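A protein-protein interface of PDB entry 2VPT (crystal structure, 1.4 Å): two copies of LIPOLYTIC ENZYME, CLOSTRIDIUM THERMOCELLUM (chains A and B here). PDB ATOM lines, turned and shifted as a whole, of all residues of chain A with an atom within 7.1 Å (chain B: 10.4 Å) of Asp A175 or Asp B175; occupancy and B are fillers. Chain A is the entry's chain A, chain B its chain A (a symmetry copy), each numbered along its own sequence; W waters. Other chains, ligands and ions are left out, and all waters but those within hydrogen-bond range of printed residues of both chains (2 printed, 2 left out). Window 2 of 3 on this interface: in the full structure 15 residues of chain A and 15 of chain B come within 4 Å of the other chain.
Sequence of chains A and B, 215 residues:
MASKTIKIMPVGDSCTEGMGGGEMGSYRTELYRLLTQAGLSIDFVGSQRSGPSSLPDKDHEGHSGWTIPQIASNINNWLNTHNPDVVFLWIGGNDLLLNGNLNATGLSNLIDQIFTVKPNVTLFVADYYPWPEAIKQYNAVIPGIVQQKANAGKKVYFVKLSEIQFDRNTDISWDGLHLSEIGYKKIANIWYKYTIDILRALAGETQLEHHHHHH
OG of Ser A173 sits at hydrogen-bond distance from OD1 of Asp A175 (2.9 Å). OG of Ser B64 lies close to SD of Met B19 (3.7 Å). A ring nitrogen (ND1) of His B178 is in hydrogen-bond range of the side-chain carboxylate (OD2) of Asp B175, at 2.8 Å. The backbone NH of Ser A173 lies within hydrogen-bond range of the backbone carbonyl oxygen of His A178, 2.8 Å away. The side-chain hydroxyl (OG) of Ser B173 sits at hydrogen-bond distance from the side-chain carboxylate (OD1) of Asp B175. The backbone NH of Met B19 is in hydrogen-bond range of the backbone carbonyl oxygen of Ser B14 (3.0 Å).
Hydrophobic or aromatic side chains of chain B within 4 Å of the printed part of chain A: Met B19, Met B24, Trp B174 and His B178. Along chain B the printed residues that touch a printed residue of chain A span positions 19 to 178. Hydrophobic or aromatic side chains of chain A within 4 Å of the printed part of chain B: Met A19, Trp A174 and His A178.
Of the printed residues of chain B, Met A19 touches Gly B20 and Met B24. Printed residues of chain B within 4 Å of Asp A175: Trp B174 (3.0 Å) and Asp B175 (3.9 Å). Gly A176 touches none of the printed residues of chain B. His A178 touches one residue of chain B. Of the printed residues of chain A, Met B19 touches Gly A20. Printed residues of chain A within 4 Å of Gly B20: Met A19. Of the printed residues of chain A, Met B24 touches Met A19 (3.4 Å). Tyr B129 touches none of the printed residues of chain A. Of chain A, only Trp A174 and Asp A175 come within 4 Å of Asp B175. Ser B180 touches none of the printed residues of chain A. The nearest residue of chain B that does not touch Asp A175 is Gly B176 (6.8 Å). The nearest residue of chain A that does not touch Asp B175 is Gly A176 (6.8 Å).
Met A19 touches Gly B20. Met A19 touches Met B24. Met B19 touches Gly A20. CH2 of Trp A174 touches OD2 of Asp B175, 3.0 Å away. His B178 touches Trp A174. CH2 of Trp B174 touches OD2 of Asp A175, at 3.0 Å. Asp A175 touches Asp B175. His A178 touches Trp B174 (CE1 to CH2, 3.4 Å).
Met A19 touches Gly B20, and with the chains exchanged Gly A20 touches Met B19. Trp A174 touches Asp B175, and with the chains exchanged Asp A175 touches Trp B174. Trp A174 touches His B178, and with the chains exchanged His A178 touches Trp B174. Asp A175 touches its own counterpart, Asp B175. Positions printed for both chains: 19, 20, 21, 131, 172, 173, 174, 175, 176, 177, 178 and 179.
Water W1 lies within hydrogen-bond range of the backbone carbonyl oxygen of Gly B20 (2.7 Å), the indole nitrogen of Trp B174 (3.2 Å) and the side-chain sulfur of Met A19 (3.5 Å). Water W2 lies within hydrogen-bond range of the backbone carbonyl oxygen (O) of Gly A20 (2.7 Å), the indole nitrogen (NE1) of Trp A174 (3.2 Å) and the side-chain sulfur (SD) of Met B19 (3.5 Å).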
ATOM      1  N   MET A  19       9.203  -5.147   7.188  1.00  0.00           N
ATOM      2  CA  MET A  19       8.819  -3.760   7.343  1.00  0.00           C
ATOM      3  C   MET A  19       9.895  -2.874   6.714  1.00  0.00           C
ATOM      4  O   MET A  19      11.047  -3.285   6.532  1.00  0.00           O
ATOM      5  CB  MET A  19       8.605  -3.401   8.812  1.00  0.00           C
ATOM      6  CG  MET A  19       7.404  -4.055   9.410  1.00  0.00           C
ATOM      7  SD  MET A  19       6.940  -3.339  11.156  1.00  0.00           S
ATOM      8  CE  MET A  19       5.115  -3.869  11.255  1.00  0.00           C
ATOM      9  N   GLY A  20       9.515  -1.654   6.364  1.00  0.00           N
ATOM     10  CA  GLY A  20      10.402  -0.746   5.641  1.00  0.00           C
ATOM     11  C   GLY A  20      10.076  -0.783   4.168  1.00  0.00           C
ATOM     12  O   GLY A  20       8.901  -0.816   3.767  1.00  0.00           O
ATOM     13  N   GLY A  21      11.119  -0.762   3.351  1.00  0.00           N
ATOM     14  CA  GLY A  21      10.947  -0.817   1.901  1.00  0.00           C
ATOM     15  C   GLY A  21      10.889  -2.238   1.386  1.00  0.00           C
ATOM     16  O   GLY A  21      11.349  -3.163   2.043  1.00  0.00           O
ATOM     17  N   TRP A 131      21.931  -0.490  13.126  1.00  0.00           N
ATOM     18  CA  TRP A 131      20.968   0.600  13.263  1.00  0.00           C
ATOM     19  C   TRP A 131      19.725   0.083  13.971  1.00  0.00           C
ATOM     20  O   TRP A 131      19.190  -0.943  13.565  1.00  0.00           O
ATOM     21  CB  TRP A 131      20.579   1.128  11.882  1.00  0.00           C
ATOM     22  CG  TRP A 131      19.787   2.388  11.938  1.00  0.00           C
ATOM     23  CD1 TRP A 131      18.449   2.522  11.782  1.00  0.00           C
ATOM     24  CD2 TRP A 131      20.300   3.700  12.182  1.00  0.00           C
ATOM     25  NE1 TRP A 131      18.087   3.840  11.900  1.00  0.00           N
ATOM     26  CE2 TRP A 131      19.210   4.585  12.144  1.00  0.00           C
ATOM     27  CE3 TRP A 131      21.581   4.212  12.416  1.00  0.00           C
ATOM     28  CZ2 TRP A 131      19.355   5.964  12.346  1.00  0.00           C
ATOM     29  CZ3 TRP A 131      21.725   5.581  12.613  1.00  0.00           C
ATOM     30  CH2 TRP A 131      20.617   6.437  12.573  1.00  0.00           C
ATOM     31  N   ILE A 172      18.231   2.809   4.836  1.00  0.00           N
ATOM     32  CA  ILE A 172      17.130   2.923   5.789  1.00  0.00           C
ATOM     33  C   ILE A 172      15.894   3.508   5.120  1.00  0.00           C
ATOM     34  O   ILE A 172      15.976   4.465   4.354  1.00  0.00           O
ATOM     35  CB  ILE A 172      17.541   3.761   7.015  1.00  0.00           C
ATOM     36  CG1 ILE A 172      18.659   3.048   7.789  1.00  0.00           C
ATOM     37  CG2 ILE A 172      16.339   4.032   7.936  1.00  0.00           C
ATOM     38  CD1 ILE A 172      18.330   1.601   8.244  1.00  0.00           C
ATOM     39  N   SER A 173      14.746   2.910   5.414  1.00  0.00           N
ATOM     40  CA  SER A 173      13.487   3.297   4.808  1.00  0.00           C
ATOM     41  C   SER A 173      12.950   4.611   5.370  1.00  0.00           C
ATOM     42  O   SER A 173      13.506   5.190   6.297  1.00  0.00           O
ATOM     43  CB  SER A 173      12.447   2.198   5.050  1.00  0.00           C
ATOM     44  OG  SER A 173      11.940   2.276   6.368  1.00  0.00           O
ATOM     45  N   TRP A 174      11.850   5.056   4.784  1.00  0.00           N
ATOM     46  CA  TRP A 174      11.119   6.234   5.243  1.00  0.00           C
ATOM     47  C   TRP A 174      10.731   6.218   6.731  1.00  0.00           C
ATOM     48  O   TRP A 174      10.522   7.279   7.320  1.00  0.00           O
ATOM     49  CB  TRP A 174       9.852   6.405   4.394  1.00  0.00           C
ATOM     50  CG  TRP A 174       8.976   5.198   4.443  1.00  0.00           C
ATOM     51  CD1 TRP A 174       9.044   4.091   3.639  1.00  0.00           C
ATOM     52  CD2 TRP A 174       7.914   4.955   5.366  1.00  0.00           C
ATOM     53  NE1 TRP A 174       8.091   3.175   4.011  1.00  0.00           N
ATOM     54  CE2 TRP A 174       7.381   3.682   5.066  1.00  0.00           C
ATOM     55  CE3 TRP A 174       7.363   5.689   6.420  1.00  0.00           C
ATOM     56  CZ2 TRP A 174       6.322   3.132   5.779  1.00  0.00           C
ATOM     57  CZ3 TRP A 174       6.308   5.140   7.123  1.00  0.00           C
ATOM     58  CH2 TRP A 174       5.801   3.875   6.799  1.00  0.00           C
ATOM     59  N   ASP A 175      10.615   5.040   7.354  1.00  0.00           N
ATOM     60  CA  ASP A 175      10.260   4.984   8.782  1.00  0.00           C
ATOM     61  C   ASP A 175      11.431   5.245   9.740  1.00  0.00           C
ATOM     62  O   ASP A 175      11.238   5.321  10.963  1.00  0.00           O
ATOM     63  CB  ASP A 175       9.489   3.688   9.140  1.00  0.00           C
ATOM     64  CG  ASP A 175      10.367   2.437   9.231  1.00  0.00           C
ATOM     65  OD1 ASP A 175      11.614   2.524   9.257  1.00  0.00           O
ATOM     66  OD2 ASP A 175       9.769   1.332   9.297  1.00  0.00           O
ATOM     67  N   GLY A 176      12.634   5.392   9.186  1.00  0.00           N
ATOM     68  CA  GLY A 176      13.810   5.747   9.965  1.00  0.00           C
ATOM     69  C   GLY A 176      14.423   4.635  10.788  1.00  0.00           C
ATOM     70  O   GLY A 176      15.381   4.873  11.509  1.00  0.00           O
ATOM     71  N   LEU A 177      13.904   3.413  10.660  1.00  0.00           N
ATOM     72  CA  LEU A 177      14.357   2.286  11.486  1.00  0.00           C
ATOM     73  C   LEU A 177      14.646   1.026  10.664  1.00  0.00           C
ATOM     74  O   LEU A 177      15.713   0.410  10.794  1.00  0.00           O
ATOM     75  CB  LEU A 177      13.285   1.976  12.529  1.00  0.00           C
ATOM     76  CG  LEU A 177      13.481   0.802  13.480  1.00  0.00           C
ATOM     77  CD1 LEU A 177      14.733   0.989  14.332  1.00  0.00           C
ATOM     78  CD2 LEU A 177      12.247   0.649  14.353  1.00  0.00           C
ATOM     79  N   HIS A 178      13.673   0.634   9.847  1.00  0.00           N
ATOM     80  CA  HIS A 178      13.778  -0.559   9.032  1.00  0.00           C
ATOM     81  C   HIS A 178      14.491  -0.271   7.727  1.00  0.00           C
ATOM     82  O   HIS A 178      14.558   0.872   7.272  1.00  0.00           O
ATOM     83  CB  HIS A 178      12.391  -1.120   8.738  1.00  0.00           C
ATOM     84  CG  HIS A 178      11.697  -1.638   9.955  1.00  0.00           C
ATOM     85  ND1 HIS A 178      10.711  -0.929  10.598  1.00  0.00           N
ATOM     86  CD2 HIS A 178      11.868  -2.780  10.658  1.00  0.00           C
ATOM     87  CE1 HIS A 178      10.292  -1.624  11.646  1.00  0.00           C
ATOM     88  NE2 HIS A 178      10.984  -2.745  11.709  1.00  0.00           N
ATOM     89  N   LEU A 179      15.017  -1.334   7.141  1.00  0.00           N
ATOM     90  CA  LEU A 179      15.756  -1.236   5.892  1.00  0.00           C
ATOM     91  C   LEU A 179      14.887  -0.797   4.717  1.00  0.00           C
ATOM     92  O   LEU A 179      13.700  -1.105   4.648  1.00  0.00           O
ATOM     93  CB  LEU A 179      16.410  -2.586   5.564  1.00  0.00           C
ATOM     94  CG  LEU A 179      17.509  -3.065   6.512  1.00  0.00           C
ATOM     95  CD1 LEU A 179      17.783  -4.526   6.242  1.00  0.00           C
ATOM     96  CD2 LEU A 179      18.783  -2.218   6.400  1.00  0.00           C
ATOM     97  N   SER B  14      -1.284  -0.651   2.242  1.00  0.00           N
ATOM     98  CA  SER B  14      -0.660  -0.929   3.530  1.00  0.00           C
ATOM     99  C   SER B  14      -1.630  -0.785   4.691  1.00  0.00           C
ATOM    100  O   SER B  14      -1.349  -1.297   5.769  1.00  0.00           O
ATOM    101  CB  SER B  14       0.568  -0.082   3.790  1.00  0.00           C
ATOM    102  OG  SER B  14       0.282   1.253   3.580  1.00  0.00           O
ATOM    103  N   CYS B  15      -2.740  -0.073   4.491  1.00  0.00           N
ATOM    104  CA  CYS B  15      -3.740   0.065   5.542  1.00  0.00           C
ATOM    105  C   CYS B  15      -4.541  -1.205   5.754  1.00  0.00           C
ATOM    106  O   CYS B  15      -5.142  -1.378   6.812  1.00  0.00           O
ATOM    107  CB  CYS B  15      -4.682   1.230   5.267  1.00  0.00           C
ATOM    108  SG  CYS B  15      -3.900   2.839   5.124  1.00  0.00           S
ATOM    109  N   GLY B  18      -1.586  -3.842   6.970  1.00  0.00           N
ATOM    110  CA  GLY B  18      -1.454  -3.501   8.386  1.00  0.00           C
ATOM    111  C   GLY B  18      -0.134  -2.927   8.844  1.00  0.00           C
ATOM    112  O   GLY B  18       0.318  -3.188   9.961  1.00  0.00           O
ATOM    113  N   MET B  19       0.510  -2.116   8.013  1.00  0.00           N
ATOM    114  CA  MET B  19       1.683  -1.410   8.483  1.00  0.00           C
ATOM    115  C   MET B  19       1.283  -0.501   9.647  1.00  0.00           C
ATOM    116  O   MET B  19       0.112  -0.141   9.813  1.00  0.00           O
ATOM    117  CB  MET B  19       2.335  -0.605   7.360  1.00  0.00           C
ATOM    118  CG  MET B  19       2.968  -1.460   6.313  1.00  0.00           C
ATOM    119  SD  MET B  19       4.081  -0.452   5.082  1.00  0.00           S
ATOM    120  CE  MET B  19       5.179  -1.853   4.407  1.00  0.00           C
ATOM    121  N   GLY B  20       2.259  -0.142  10.468  1.00  0.00           N
ATOM    122  CA  GLY B  20       2.001   0.618  11.688  1.00  0.00           C
ATOM    123  C   GLY B  20       1.959  -0.317  12.871  1.00  0.00           C
ATOM    124  O   GLY B  20       2.770  -1.251  12.984  1.00  0.00           O
ATOM    125  N   GLY B  21       1.021  -0.061  13.771  1.00  0.00           N
ATOM    126  CA  GLY B  21       0.855  -0.903  14.953  1.00  0.00           C
ATOM    127  C   GLY B  21      -0.064  -2.076  14.695  1.00  0.00           C
ATOM    128  O   GLY B  21      -0.865  -2.053  13.769  1.00  0.00           O
ATOM    129  N   GLY B  22       0.062  -3.109  15.520  1.00  0.00           N
ATOM    130  CA  GLY B  22      -0.820  -4.257  15.470  1.00  0.00           C
ATOM    131  C   GLY B  22      -0.317  -5.518  14.787  1.00  0.00           C
ATOM    132  O   GLY B  22      -1.107  -6.379  14.465  1.00  0.00           O
ATOM    133  N   MET B  24       0.753  -6.350  11.830  1.00  0.00           N
ATOM    134  CA  MET B  24       0.266  -6.634  10.479  1.00  0.00           C
ATOM    135  C   MET B  24      -1.106  -7.295  10.469  1.00  0.00           C
ATOM    136  O   MET B  24      -1.437  -8.094   9.596  1.00  0.00           O
ATOM    137  CB  MET B  24       1.295  -7.434   9.673  1.00  0.00           C
ATOM    138  CG  MET B  24       2.718  -6.901   9.724  1.00  0.00           C
ATOM    139  SD  MET B  24       3.014  -5.171   8.884  1.00  0.00           S
ATOM    140  CE  MET B  24       2.176  -5.626   7.510  1.00  0.00           C
ATOM    141  N   SER B  64       0.898  -3.596   0.692  1.00  0.00           N
ATOM    142  CA  SER B  64       1.584  -2.357   0.983  1.00  0.00           C
ATOM    143  C   SER B  64       2.235  -1.814  -0.280  1.00  0.00           C
ATOM    144  O   SER B  64       2.883  -2.547  -1.014  1.00  0.00           O
ATOM    145  CB  SER B  64       2.644  -2.572   2.059  1.00  0.00           C
ATOM    146  OG  SER B  64       2.038  -3.007   3.261  1.00  0.00           O
ATOM    147  N   TYR B 129      -8.937   7.501   6.966  1.00  0.00           N
ATOM    148  CA  TYR B 129      -8.749   8.386   8.109  1.00  0.00           C
ATOM    149  C   TYR B 129      -7.989   9.621   7.596  1.00  0.00           C
ATOM    150  O   TYR B 129      -7.217   9.532   6.646  1.00  0.00           O
ATOM    151  CB  TYR B 129      -7.996   7.668   9.239  1.00  0.00           C
ATOM    152  CG  TYR B 129      -6.674   7.073   8.828  1.00  0.00           C
ATOM    153  CD1 TYR B 129      -5.499   7.788   8.985  1.00  0.00           C
ATOM    154  CD2 TYR B 129      -6.603   5.801   8.251  1.00  0.00           C
ATOM    155  CE1 TYR B 129      -4.283   7.267   8.595  1.00  0.00           C
ATOM    156  CE2 TYR B 129      -5.389   5.269   7.849  1.00  0.00           C
ATOM    157  CZ  TYR B 129      -4.229   6.002   8.028  1.00  0.00           C
ATOM    158  OH  TYR B 129      -3.004   5.482   7.650  1.00  0.00           O
ATOM    159  N   TRP B 131      -5.343  11.464   7.511  1.00  0.00           N
ATOM    160  CA  TRP B 131      -3.911  11.622   7.747  1.00  0.00           C
ATOM    161  C   TRP B 131      -3.141  10.880   6.663  1.00  0.00           C
ATOM    162  O   TRP B 131      -3.433   9.715   6.416  1.00  0.00           O
ATOM    163  CB  TRP B 131      -3.540  11.044   9.113  1.00  0.00           C
ATOM    164  CG  TRP B 131      -2.149  11.374   9.531  1.00  0.00           C
ATOM    165  CD1 TRP B 131      -1.066  10.563   9.485  1.00  0.00           C
ATOM    166  CD2 TRP B 131      -1.695  12.627  10.051  1.00  0.00           C
ATOM    167  NE1 TRP B 131       0.041  11.222   9.956  1.00  0.00           N
ATOM    168  CE2 TRP B 131      -0.321  12.493  10.313  1.00  0.00           C
ATOM    169  CE3 TRP B 131      -2.324  13.844  10.332  1.00  0.00           C
ATOM    170  CZ2 TRP B 131       0.448  13.542  10.834  1.00  0.00           C
ATOM    171  CZ3 TRP B 131      -1.561  14.882  10.852  1.00  0.00           C
ATOM    172  CH2 TRP B 131      -0.191  14.720  11.099  1.00  0.00           C
ATOM    173  N   PRO B 132      -2.201  11.557   5.973  1.00  0.00           N
ATOM    174  CA  PRO B 132      -1.891  12.983   6.048  1.00  0.00           C
ATOM    175  C   PRO B 132      -3.075  13.822   5.571  1.00  0.00           C
ATOM    176  O   PRO B 132      -3.960  13.307   4.886  1.00  0.00           O
ATOM    177  CB  PRO B 132      -0.702  13.138   5.092  1.00  0.00           C
ATOM    178  CG  PRO B 132      -0.822  12.018   4.156  1.00  0.00           C
ATOM    179  CD  PRO B 132      -1.383  10.883   4.951  1.00  0.00           C
ATOM    180  N   ARG B 168      -4.230  12.285  16.587  1.00  0.00           N
ATOM    181  CA  ARG B 168      -2.878  11.955  16.144  1.00  0.00           C
ATOM    182  C   ARG B 168      -1.978  11.431  17.265  1.00  0.00           C
ATOM    183  O   ARG B 168      -1.041  10.668  17.001  1.00  0.00           O
ATOM    184  CB  ARG B 168      -2.240  13.177  15.471  1.00  0.00           C
ATOM    185  CG  ARG B 168      -2.131  14.407  16.378  1.00  0.00           C
ATOM    186  CD  ARG B 168      -2.654  15.685  15.710  1.00  0.00           C
ATOM    187  NE  ARG B 168      -4.019  15.547  15.182  1.00  0.00           N
ATOM    188  CZ  ARG B 168      -5.128  15.481  15.921  1.00  0.00           C
ATOM    189  NH1 ARG B 168      -5.077  15.517  17.248  1.00  0.00           N
ATOM    190  NH2 ARG B 168      -6.305  15.365  15.322  1.00  0.00           N
ATOM    191  N   ASP B 171      -3.735   7.613  17.638  1.00  0.00           N
ATOM    192  CA  ASP B 171      -4.177   6.799  16.503  1.00  0.00           C
ATOM    193  C   ASP B 171      -3.121   6.555  15.439  1.00  0.00           C
ATOM    194  O   ASP B 171      -3.352   5.760  14.531  1.00  0.00           O
ATOM    195  CB  ASP B 171      -5.383   7.470  15.847  1.00  0.00           C
ATOM    196  CG  ASP B 171      -6.561   7.608  16.799  1.00  0.00           C
ATOM    197  OD1 ASP B 171      -6.560   6.936  17.850  1.00  0.00           O
ATOM    198  OD2 ASP B 171      -7.502   8.363  16.481  1.00  0.00           O
ATOM    199  N   ILE B 172      -1.991   7.246  15.527  1.00  0.00           N
ATOM    200  CA  ILE B 172      -0.900   7.103  14.567  1.00  0.00           C
ATOM    201  C   ILE B 172       0.287   6.388  15.197  1.00  0.00           C
ATOM    202  O   ILE B 172       0.670   6.666  16.330  1.00  0.00           O
ATOM    203  CB  ILE B 172      -0.479   8.473  13.998  1.00  0.00           C
ATOM    204  CG1 ILE B 172      -1.634   9.087  13.194  1.00  0.00           C
ATOM    205  CG2 ILE B 172       0.779   8.351  13.122  1.00  0.00           C
ATOM    206  CD1 ILE B 172      -2.184   8.201  12.044  1.00  0.00           C
ATOM    207  N   SER B 173       0.857   5.453  14.445  1.00  0.00           N
ATOM    208  CA  SER B 173       1.952   4.631  14.921  1.00  0.00           C
ATOM    209  C   SER B 173       3.272   5.395  14.979  1.00  0.00           C
ATOM    210  O   SER B 173       3.368   6.547  14.567  1.00  0.00           O
ATOM    211  CB  SER B 173       2.123   3.424  13.993  1.00  0.00           C
ATOM    212  OG  SER B 173       2.801   3.801  12.810  1.00  0.00           O
ATOM    213  N   TRP B 174       4.284   4.716  15.495  1.00  0.00           N
ATOM    214  CA  TRP B 174       5.652   5.227  15.539  1.00  0.00           C
ATOM    215  C   TRP B 174       6.212   5.699  14.188  1.00  0.00           C
ATOM    216  O   TRP B 174       7.130   6.519  14.159  1.00  0.00           O
ATOM    217  CB  TRP B 174       6.575   4.146  16.117  1.00  0.00           C
ATOM    218  CG  TRP B 174       6.519   2.879  15.331  1.00  0.00           C
ATOM    219  CD1 TRP B 174       5.642   1.840  15.496  1.00  0.00           C
ATOM    220  CD2 TRP B 174       7.356   2.524  14.230  1.00  0.00           C
ATOM    221  NE1 TRP B 174       5.882   0.864  14.559  1.00  0.00           N
ATOM    222  CE2 TRP B 174       6.932   1.257  13.773  1.00  0.00           C
ATOM    223  CE3 TRP B 174       8.421   3.155  13.582  1.00  0.00           C
ATOM    224  CZ2 TRP B 174       7.539   0.610  12.704  1.00  0.00           C
ATOM    225  CZ3 TRP B 174       9.025   2.507  12.524  1.00  0.00           C
ATOM    226  CH2 TRP B 174       8.581   1.249  12.094  1.00  0.00           C
ATOM    227  N   ASP B 175       5.693   5.194  13.063  1.00  0.00           N
ATOM    228  CA  ASP B 175       6.193   5.633  11.749  1.00  0.00           C
ATOM    229  C   ASP B 175       5.627   6.977  11.270  1.00  0.00           C
ATOM    230  O   ASP B 175       6.045   7.499  10.224  1.00  0.00           O
ATOM    231  CB  ASP B 175       6.057   4.525  10.675  1.00  0.00           C
ATOM    232  CG  ASP B 175       4.632   4.324  10.150  1.00  0.00           C
ATOM    233  OD1 ASP B 175       3.731   5.155  10.398  1.00  0.00           O
ATOM    234  OD2 ASP B 175       4.428   3.300   9.450  1.00  0.00           O
ATOM    235  N   GLY B 176       4.690   7.537  12.034  1.00  0.00           N
ATOM    236  CA  GLY B 176       4.145   8.858  11.754  1.00  0.00           C
ATOM    237  C   GLY B 176       3.143   8.936  10.623  1.00  0.00           C
ATOM    238  O   GLY B 176       2.684  10.020  10.296  1.00  0.00           O
ATOM    239  N   LEU B 177       2.771   7.793  10.046  1.00  0.00           N
ATOM    240  CA  LEU B 177       1.883   7.766   8.876  1.00  0.00           C
ATOM    241  C   LEU B 177       0.738   6.758   9.022  1.00  0.00           C
ATOM    242  O   LEU B 177      -0.436   7.090   8.808  1.00  0.00           O
ATOM    243  CB  LEU B 177       2.707   7.421   7.639  1.00  0.00           C
ATOM    244  CG  LEU B 177       2.011   7.268   6.292  1.00  0.00           C
ATOM    245  CD1 LEU B 177       1.318   8.563   5.881  1.00  0.00           C
ATOM    246  CD2 LEU B 177       3.026   6.839   5.245  1.00  0.00           C
ATOM    247  N   HIS B 178       1.098   5.522   9.355  1.00  0.00           N
ATOM    248  CA  HIS B 178       0.137   4.445   9.493  1.00  0.00           C
ATOM    249  C   HIS B 178      -0.473   4.430  10.879  1.00  0.00           C
ATOM    250  O   HIS B 178       0.093   4.965  11.835  1.00  0.00           O
ATOM    251  CB  HIS B 178       0.807   3.103   9.220  1.00  0.00           C
ATOM    252  CG  HIS B 178       1.245   2.944   7.802  1.00  0.00           C
ATOM    253  ND1 HIS B 178       2.555   3.094   7.414  1.00  0.00           N
ATOM    254  CD2 HIS B 178       0.543   2.676   6.678  1.00  0.00           C
ATOM    255  CE1 HIS B 178       2.644   2.911   6.105  1.00  0.00           C
ATOM    256  NE2 HIS B 178       1.436   2.664   5.634  1.00  0.00           N
ATOM    257  N   LEU B 179      -1.635   3.805  10.962  1.00  0.00           N
ATOM    258  CA  LEU B 179      -2.372   3.714  12.213  1.00  0.00           C
ATOM    259  C   LEU B 179      -1.649   2.886  13.273  1.00  0.00           C
ATOM    260  O   LEU B 179      -0.937   1.933  12.965  1.00  0.00           O
ATOM    261  CB  LEU B 179      -3.762   3.111  11.959  1.00  0.00           C
ATOM    262  CG  LEU B 179      -4.728   3.944  11.116  1.00  0.00           C
ATOM    263  CD1 LEU B 179      -5.881   3.069  10.690  1.00  0.00           C
ATOM    264  CD2 LEU B 179      -5.208   5.201  11.856  1.00  0.00           C
ATOM    265  N   SER B 180      -1.872   3.266  14.531  1.00  0.00           N
ATOM    266  CA  SER B 180      -1.514   2.452  15.680  1.00  0.00           C
ATOM    267  C   SER B 180      -2.529   1.334  15.889  1.00  0.00           C
ATOM    268  O   SER B 180      -3.568   1.276  15.223  1.00  0.00           O
ATOM    269  CB  SER B 180      -1.536   3.325  16.923  1.00  0.00           C
ATOM    270  OG  SER B 180      -2.861   3.786  17.131  1.00  0.00           O
ATOM    271  N   GLU B 181      -2.268   0.455  16.854  1.00  0.00           N
ATOM    272  CA  GLU B 181      -3.233  -0.565  17.219  1.00  0.00           C
ATOM    273  C   GLU B 181      -4.579   0.055  17.621  1.00  0.00           C
ATOM    274  O   GLU B 181      -5.640  -0.429  17.233  1.00  0.00           O
ATOM    275  CB  GLU B 181      -2.658  -1.412  18.357  1.00  0.00           C
ATOM    276  CG  GLU B 181      -3.353  -2.710  18.626  1.00  0.00           C
ATOM    277  CD  GLU B 181      -2.493  -3.610  19.510  1.00  0.00           C
ATOM    278  OE1 GLU B 181      -2.080  -3.145  20.589  1.00  0.00           O
ATOM    279  OE2 GLU B 181      -2.203  -4.764  19.121  1.00  0.00           O
ATOM    280  N   TYR B 184      -6.333   1.321  14.470  1.00  0.00           N
ATOM    281  CA  TYR B 184      -6.952   0.227  13.745  1.00  0.00           C
ATOM    282  C   TYR B 184      -8.225  -0.289  14.416  1.00  0.00           C
ATOM    283  O   TYR B 184      -9.157  -0.706  13.741  1.00  0.00           O
ATOM    284  CB  TYR B 184      -5.971  -0.923  13.502  1.00  0.00           C
ATOM    285  CG  TYR B 184      -5.015  -0.710  12.345  1.00  0.00           C
ATOM    286  CD1 TYR B 184      -5.498  -0.523  11.067  1.00  0.00           C
ATOM    287  CD2 TYR B 184      -3.645  -0.783  12.515  1.00  0.00           C
ATOM    288  CE1 TYR B 184      -4.637  -0.370   9.978  1.00  0.00           C
ATOM    289  CE2 TYR B 184      -2.778  -0.615  11.451  1.00  0.00           C
ATOM    290  CZ  TYR B 184      -3.278  -0.406  10.180  1.00  0.00           C
ATOM    291  OH  TYR B 184      -2.421  -0.256   9.086  1.00  0.00           O
HETATM  292  O   HOH W   1       5.109  -2.137  13.870  1.00  0.00           O
HETATM  293  O   HOH W   2       6.722   0.493   3.006  1.00  0.00           O
